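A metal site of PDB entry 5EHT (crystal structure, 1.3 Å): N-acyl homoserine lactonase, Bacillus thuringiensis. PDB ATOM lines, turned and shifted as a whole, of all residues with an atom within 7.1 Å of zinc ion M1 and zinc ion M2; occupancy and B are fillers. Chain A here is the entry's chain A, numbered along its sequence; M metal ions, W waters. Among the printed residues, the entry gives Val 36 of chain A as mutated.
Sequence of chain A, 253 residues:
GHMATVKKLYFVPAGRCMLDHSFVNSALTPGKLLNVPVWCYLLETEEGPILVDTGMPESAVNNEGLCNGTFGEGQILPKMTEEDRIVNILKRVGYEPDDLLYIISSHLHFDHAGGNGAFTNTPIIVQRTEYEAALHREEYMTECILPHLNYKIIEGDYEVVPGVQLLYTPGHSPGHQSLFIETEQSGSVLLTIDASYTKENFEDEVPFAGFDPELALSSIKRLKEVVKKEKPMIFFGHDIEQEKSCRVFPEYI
ND1 of His 112 is in hydrogen-bond range of OG of Ser 106. The side-chain carboxylate (OD2) of Asp 53 is in hydrogen-bond range of a ring nitrogen (ND1) of His 112, 2.8 Å away. The backbone carbonyl oxygen (O) of Ala 209 lies within hydrogen-bond range of a ring nitrogen (ND1) of His 172. NE2 of His 176 is in hydrogen-bond range of N of Asp 194 (3.0 Å). N of His 238 is in hydrogen-bond range of O of Tyr 197 (2.8 Å). A ring nitrogen (ND1) of His 238 lies within hydrogen-bond range of the backbone carbonyl oxygen (O) of Pro 37. A ring nitrogen (ND1) of His 107 is in hydrogen-bond range of the side-chain hydroxyl of Ser 106.
Four residues have an atom within 4 Å of zinc ion M1: His 107, His 109, His 172 and Asp 194.
Zinc ion M1 is bound by water W1 (2.0 Å), a ring nitrogen (NE2) of His 172 (2.1 Å), a ring nitrogen (NE2) of His 107 (2.1 Å), a ring nitrogen (ND1) of His 109 (2.1 Å) and the side-chain carboxylate of Asp 194 (2.6 Å). Zinc ion M1 has five donor atoms within binding distance.
NE2 of His 112 binds zinc ion M2 (2.0 Å). The side-chain carboxylate (OD2) of Asp 194 binds zinc ion M2 (2.1 Å). Zinc ion M2 is bound by water W1 (2.1 Å). Zinc ion M2 is bound by NE2 of His 238 (2.1 Å). Zinc ion M2 is bound by OD2 of Asp 111. Zinc ion M2 has five donor atoms within binding distance.
Four residues have an atom within 4 Å of zinc ion M2: Asp 111, His 112, Asp 194 and His 238. The nearest printed residue that does not touch zinc ion M2 is His 107 (4.2 Å).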
ATOM      1  N   LEU A  19       7.150 -13.099 -18.343  1.00  0.00           N
ATOM      2  CA  LEU A  19       7.092 -12.308 -19.547  1.00  0.00           C
ATOM      3  C   LEU A  19       7.822 -10.985 -19.290  1.00  0.00           C
ATOM      4  O   LEU A  19       7.596 -10.335 -18.278  1.00  0.00           O
ATOM      5  CB  LEU A  19       5.667 -11.956 -20.011  1.00  0.00           C
ATOM      6  CG  LEU A  19       4.799 -13.133 -20.455  1.00  0.00           C
ATOM      7  CD1 LEU A  19       3.398 -12.601 -20.772  1.00  0.00           C
ATOM      8  CD2 LEU A  19       5.450 -13.930 -21.588  1.00  0.00           C
ATOM      9  N   VAL A  36       3.505 -14.035 -14.676  1.00  0.00           N
ATOM     10  CA  VAL A  36       2.084 -13.911 -14.982  1.00  0.00           C
ATOM     11  C   VAL A  36       1.434 -15.299 -14.864  1.00  0.00           C
ATOM     12  O   VAL A  36       2.023 -16.350 -15.051  1.00  0.00           O
ATOM     13  CB  VAL A  36       1.800 -13.317 -16.362  1.00  0.00           C
ATOM     14  CG1 VAL A  36       2.452 -11.961 -16.545  1.00  0.00           C
ATOM     15  CG2 VAL A  36       2.141 -14.248 -17.495  1.00  0.00           C
ATOM     16  N   PRO A  37       0.101 -15.286 -14.537  1.00  0.00           N
ATOM     17  CA  PRO A  37      -0.611 -16.536 -14.449  1.00  0.00           C
ATOM     18  C   PRO A  37      -0.865 -17.154 -15.810  1.00  0.00           C
ATOM     19  O   PRO A  37      -1.051 -16.434 -16.789  1.00  0.00           O
ATOM     20  CB  PRO A  37      -1.958 -16.215 -13.828  1.00  0.00           C
ATOM     21  CG  PRO A  37      -2.135 -14.778 -14.195  1.00  0.00           C
ATOM     22  CD  PRO A  37      -0.747 -14.159 -14.174  1.00  0.00           C
ATOM     23  N   VAL A  38      -0.841 -18.476 -15.899  1.00  0.00           N
ATOM     24  CA  VAL A  38      -1.372 -19.203 -17.006  1.00  0.00           C
ATOM     25  C   VAL A  38      -2.618 -19.882 -16.534  1.00  0.00           C
ATOM     26  O   VAL A  38      -2.650 -20.528 -15.464  1.00  0.00           O
ATOM     27  CB  VAL A  38      -0.313 -20.183 -17.564  1.00  0.00           C
ATOM     28  CG1 VAL A  38      -0.936 -21.149 -18.604  1.00  0.00           C
ATOM     29  CG2 VAL A  38       0.893 -19.468 -18.065  1.00  0.00           C
ATOM     30  N   ASP A  53      -8.596 -24.168 -23.069  1.00  0.00           N
ATOM     31  CA  ASP A  53      -7.146 -24.204 -23.109  1.00  0.00           C
ATOM     32  C   ASP A  53      -6.571 -25.338 -22.238  1.00  0.00           C
ATOM     33  O   ASP A  53      -7.215 -25.946 -21.441  1.00  0.00           O
ATOM     34  CB  ASP A  53      -6.581 -22.815 -22.770  1.00  0.00           C
ATOM     35  CG  ASP A  53      -6.891 -21.768 -23.887  1.00  0.00           C
ATOM     36  OD1 ASP A  53      -7.197 -22.211 -25.010  1.00  0.00           O
ATOM     37  OD2 ASP A  53      -6.762 -20.562 -23.584  1.00  0.00           O
ATOM     38  N   SER A 106      -8.462 -21.148 -27.298  1.00  0.00           N
ATOM     39  CA  SER A 106      -8.567 -19.702 -27.556  1.00  0.00           C
ATOM     40  C   SER A 106      -7.661 -19.349 -28.671  1.00  0.00           C
ATOM     41  O   SER A 106      -7.965 -18.511 -29.539  1.00  0.00           O
ATOM     42  CB  SER A 106      -8.243 -18.924 -26.308  1.00  0.00           C
ATOM     43  OG  SER A 106      -6.868 -19.151 -25.921  1.00  0.00           O
ATOM     44  N   HIS A 107      -6.456 -19.910 -28.696  1.00  0.00           N
ATOM     45  CA  HIS A 107      -5.465 -19.754 -29.707  1.00  0.00           C
ATOM     46  C   HIS A 107      -4.358 -20.825 -29.445  1.00  0.00           C
ATOM     47  O   HIS A 107      -4.462 -21.558 -28.452  1.00  0.00           O
ATOM     48  CB  HIS A 107      -4.917 -18.317 -29.723  1.00  0.00           C
ATOM     49  CG  HIS A 107      -4.192 -17.839 -28.538  1.00  0.00           C
ATOM     50  ND1 HIS A 107      -4.728 -17.816 -27.264  1.00  0.00           N
ATOM     51  CD2 HIS A 107      -3.009 -17.174 -28.447  1.00  0.00           C
ATOM     52  CE1 HIS A 107      -3.928 -17.156 -26.461  1.00  0.00           C
ATOM     53  NE2 HIS A 107      -2.868 -16.783 -27.134  1.00  0.00           N
ATOM     54  N   LEU A 108      -3.405 -20.873 -30.344  1.00  0.00           N
ATOM     55  CA  LEU A 108      -2.461 -21.984 -30.331  1.00  0.00           C
ATOM     56  C   LEU A 108      -1.067 -21.602 -29.808  1.00  0.00           C
ATOM     57  O   LEU A 108      -0.106 -22.329 -30.001  1.00  0.00           O
ATOM     58  CB  LEU A 108      -2.405 -22.700 -31.660  1.00  0.00           C
ATOM     59  CG  LEU A 108      -3.717 -23.390 -32.101  1.00  0.00           C
ATOM     60  CD1 LEU A 108      -3.605 -23.916 -33.512  1.00  0.00           C
ATOM     61  CD2 LEU A 108      -4.211 -24.429 -31.090  1.00  0.00           C
ATOM     62  N   HIS A 109      -0.900 -20.477 -29.135  1.00  0.00           N
ATOM     63  CA  HIS A 109       0.300 -20.173 -28.412  1.00  0.00           C
ATOM     64  C   HIS A 109       0.593 -21.253 -27.385  1.00  0.00           C
ATOM     65  O   HIS A 109      -0.340 -21.937 -26.885  1.00  0.00           O
ATOM     66  CB  HIS A 109       0.212 -18.819 -27.698  1.00  0.00           C
ATOM     67  CG  HIS A 109       0.273 -17.671 -28.645  1.00  0.00           C
ATOM     68  ND1 HIS A 109      -0.012 -16.398 -28.249  1.00  0.00           N
ATOM     69  CD2 HIS A 109       0.561 -17.626 -29.960  1.00  0.00           C
ATOM     70  CE1 HIS A 109       0.142 -15.591 -29.294  1.00  0.00           C
ATOM     71  NE2 HIS A 109       0.481 -16.308 -30.338  1.00  0.00           N
ATOM     72  N   PHE A 110       1.865 -21.415 -27.080  1.00  0.00           N
ATOM     73  CA  PHE A 110       2.326 -22.571 -26.281  1.00  0.00           C
ATOM     74  C   PHE A 110       1.721 -22.627 -24.894  1.00  0.00           C
ATOM     75  O   PHE A 110       1.612 -23.728 -24.332  1.00  0.00           O
ATOM     76  CB  PHE A 110       3.872 -22.636 -26.218  1.00  0.00           C
ATOM     77  CG  PHE A 110       4.469 -21.770 -25.166  1.00  0.00           C
ATOM     78  CD1 PHE A 110       4.456 -20.384 -25.219  1.00  0.00           C
ATOM     79  CD2 PHE A 110       4.965 -22.349 -24.083  1.00  0.00           C
ATOM     80  CE1 PHE A 110       4.954 -19.629 -24.138  1.00  0.00           C
ATOM     81  CE2 PHE A 110       5.499 -21.630 -23.058  1.00  0.00           C
ATOM     82  CZ  PHE A 110       5.484 -20.268 -23.062  1.00  0.00           C
ATOM     83  N   ASP A 111       1.344 -21.464 -24.331  1.00  0.00           N
ATOM     84  CA  ASP A 111       0.769 -21.402 -23.023  1.00  0.00           C
ATOM     85  C   ASP A 111      -0.754 -21.657 -23.025  1.00  0.00           C
ATOM     86  O   ASP A 111      -1.335 -21.673 -21.941  1.00  0.00           O
ATOM     87  CB  ASP A 111       1.138 -20.067 -22.309  1.00  0.00           C
ATOM     88  CG  ASP A 111       0.696 -18.804 -23.091  1.00  0.00           C
ATOM     89  OD1 ASP A 111       0.985 -18.770 -24.340  1.00  0.00           O
ATOM     90  OD2 ASP A 111       0.084 -17.828 -22.485  1.00  0.00           O
ATOM     91  N   HIS A 112      -1.332 -21.928 -24.182  1.00  0.00           N
ATOM     92  CA  HIS A 112      -2.746 -22.213 -24.321  1.00  0.00           C
ATOM     93  C   HIS A 112      -3.031 -23.541 -24.955  1.00  0.00           C
ATOM     94  O   HIS A 112      -4.135 -24.094 -24.720  1.00  0.00           O
ATOM     95  CB  HIS A 112      -3.424 -21.091 -25.181  1.00  0.00           C
ATOM     96  CG  HIS A 112      -3.308 -19.766 -24.499  1.00  0.00           C
ATOM     97  ND1 HIS A 112      -4.285 -19.260 -23.698  1.00  0.00           N
ATOM     98  CD2 HIS A 112      -2.258 -18.905 -24.385  1.00  0.00           C
ATOM     99  CE1 HIS A 112      -3.850 -18.134 -23.135  1.00  0.00           C
ATOM    100  NE2 HIS A 112      -2.611 -17.898 -23.540  1.00  0.00           N
ATOM    101  N   HIS A 172      -4.100 -10.403 -31.289  1.00  0.00           N
ATOM    102  CA  HIS A 172      -3.028 -10.979 -30.481  1.00  0.00           C
ATOM    103  C   HIS A 172      -2.411 -12.187 -31.212  1.00  0.00           C
ATOM    104  O   HIS A 172      -1.167 -12.344 -31.233  1.00  0.00           O
ATOM    105  CB  HIS A 172      -3.564 -11.421 -29.164  1.00  0.00           C
ATOM    106  CG  HIS A 172      -2.569 -12.240 -28.360  1.00  0.00           C
ATOM    107  ND1 HIS A 172      -1.417 -11.723 -27.791  1.00  0.00           N
ATOM    108  CD2 HIS A 172      -2.607 -13.532 -28.016  1.00  0.00           C
ATOM    109  CE1 HIS A 172      -0.770 -12.735 -27.170  1.00  0.00           C
ATOM    110  NE2 HIS A 172      -1.461 -13.810 -27.273  1.00  0.00           N
ATOM    111  N   SER A 173      -3.265 -13.003 -31.836  1.00  0.00           N
ATOM    112  CA  SER A 173      -2.848 -14.061 -32.737  1.00  0.00           C
ATOM    113  C   SER A 173      -3.827 -13.998 -33.946  1.00  0.00           C
ATOM    114  O   SER A 173      -4.906 -13.383 -33.812  1.00  0.00           O
ATOM    115  CB  SER A 173      -2.839 -15.458 -32.057  1.00  0.00           C
ATOM    116  OG  SER A 173      -4.161 -15.859 -31.795  1.00  0.00           O
ATOM    117  N   HIS A 176      -7.311 -15.646 -32.795  1.00  0.00           N
ATOM    118  CA  HIS A 176      -7.668 -15.633 -31.404  1.00  0.00           C
ATOM    119  C   HIS A 176      -9.159 -15.518 -31.182  1.00  0.00           C
ATOM    120  O   HIS A 176      -9.804 -14.736 -31.920  1.00  0.00           O
ATOM    121  CB  HIS A 176      -6.930 -14.455 -30.714  1.00  0.00           C
ATOM    122  CG  HIS A 176      -7.173 -14.394 -29.258  1.00  0.00           C
ATOM    123  ND1 HIS A 176      -8.271 -13.842 -28.655  1.00  0.00           N
ATOM    124  CD2 HIS A 176      -6.444 -14.921 -28.232  1.00  0.00           C
ATOM    125  CE1 HIS A 176      -8.225 -14.077 -27.351  1.00  0.00           C
ATOM    126  NE2 HIS A 176      -7.093 -14.715 -27.065  1.00  0.00           N
ATOM    127  N   ILE A 193      -9.496 -13.772 -22.597  1.00  0.00           N
ATOM    128  CA  ILE A 193      -8.263 -14.503 -22.919  1.00  0.00           C
ATOM    129  C   ILE A 193      -7.248 -13.421 -23.308  1.00  0.00           C
ATOM    130  O   ILE A 193      -7.136 -12.381 -22.623  1.00  0.00           O
ATOM    131  CB  ILE A 193      -8.421 -15.694 -23.859  1.00  0.00           C
ATOM    132  CG1 ILE A 193      -9.732 -16.466 -23.641  1.00  0.00           C
ATOM    133  CG2 ILE A 193      -7.197 -16.578 -23.696  1.00  0.00           C
ATOM    134  CD1 ILE A 193      -9.873 -17.184 -22.300  1.00  0.00           C
ATOM    135  N   ASP A 194      -6.488 -13.655 -24.369  1.00  0.00           N
ATOM    136  CA  ASP A 194      -5.364 -12.755 -24.705  1.00  0.00           C
ATOM    137  C   ASP A 194      -5.765 -11.627 -25.684  1.00  0.00           C
ATOM    138  O   ASP A 194      -4.879 -10.956 -26.233  1.00  0.00           O
ATOM    139  CB  ASP A 194      -4.124 -13.514 -25.156  1.00  0.00           C
ATOM    140  CG  ASP A 194      -3.444 -14.348 -24.046  1.00  0.00           C
ATOM    141  OD1 ASP A 194      -4.000 -14.359 -22.948  1.00  0.00           O
ATOM    142  OD2 ASP A 194      -2.442 -15.018 -24.458  1.00  0.00           O
ATOM    143  N   TYR A 197      -4.188  -8.780 -22.254  1.00  0.00           N
ATOM    144  CA  TYR A 197      -3.459  -9.437 -21.118  1.00  0.00           C
ATOM    145  C   TYR A 197      -3.920  -8.878 -19.815  1.00  0.00           C
ATOM    146  O   TYR A 197      -4.066  -9.613 -18.830  1.00  0.00           O
ATOM    147  CB  TYR A 197      -1.969  -9.159 -21.246  1.00  0.00           C
ATOM    148  CG  TYR A 197      -1.203  -9.934 -22.274  1.00  0.00           C
ATOM    149  CD1 TYR A 197      -1.657 -11.064 -22.957  1.00  0.00           C
ATOM    150  CD2 TYR A 197       0.027  -9.516 -22.551  1.00  0.00           C
ATOM    151  CE1 TYR A 197      -0.832 -11.787 -23.796  1.00  0.00           C
ATOM    152  CE2 TYR A 197       0.859 -10.245 -23.387  1.00  0.00           C
ATOM    153  CZ  TYR A 197       0.458 -11.377 -23.972  1.00  0.00           C
ATOM    154  OH  TYR A 197       1.286 -12.086 -24.761  1.00  0.00           O
ATOM    155  N   ALA A 209       1.659  -7.387 -26.512  1.00  0.00           N
ATOM    156  CA  ALA A 209       2.247  -8.267 -27.520  1.00  0.00           C
ATOM    157  C   ALA A 209       1.126  -8.836 -28.408  1.00  0.00           C
ATOM    158  O   ALA A 209       0.101  -9.309 -27.912  1.00  0.00           O
ATOM    159  CB  ALA A 209       2.966  -9.373 -26.868  1.00  0.00           C
ATOM    160  N   GLY A 237      -6.439 -11.990 -19.566  1.00  0.00           N
ATOM    161  CA  GLY A 237      -5.642 -13.174 -19.840  1.00  0.00           C
ATOM    162  C   GLY A 237      -4.453 -13.453 -18.917  1.00  0.00           C
ATOM    163  O   GLY A 237      -4.177 -14.616 -18.592  1.00  0.00           O
ATOM    164  N   HIS A 238      -3.670 -12.424 -18.612  1.00  0.00           N
ATOM    165  CA  HIS A 238      -2.399 -12.589 -17.914  1.00  0.00           C
ATOM    166  C   HIS A 238      -2.181 -11.415 -17.010  1.00  0.00           C
ATOM    167  O   HIS A 238      -1.256 -10.623 -17.223  1.00  0.00           O
ATOM    168  CB  HIS A 238      -1.249 -12.776 -18.923  1.00  0.00           C
ATOM    169  CG  HIS A 238      -1.249 -13.987 -19.780  1.00  0.00           C
ATOM    170  ND1 HIS A 238      -1.119 -15.264 -19.307  1.00  0.00           N
ATOM    171  CD2 HIS A 238      -1.325 -14.097 -21.113  1.00  0.00           C
ATOM    172  CE1 HIS A 238      -1.069 -16.092 -20.321  1.00  0.00           C
ATOM    173  NE2 HIS A 238      -1.199 -15.393 -21.430  1.00  0.00           N
HETATM  174 ZN    ZN M   1      -1.143 -15.718 -26.566  1.00  0.00          ZN
HETATM  175 ZN    ZN M   2      -1.339 -16.315 -23.288  1.00  0.00          ZN
HETATM  176  O   HOH W   1      -0.103 -16.142 -24.937  1.00  0.00           O
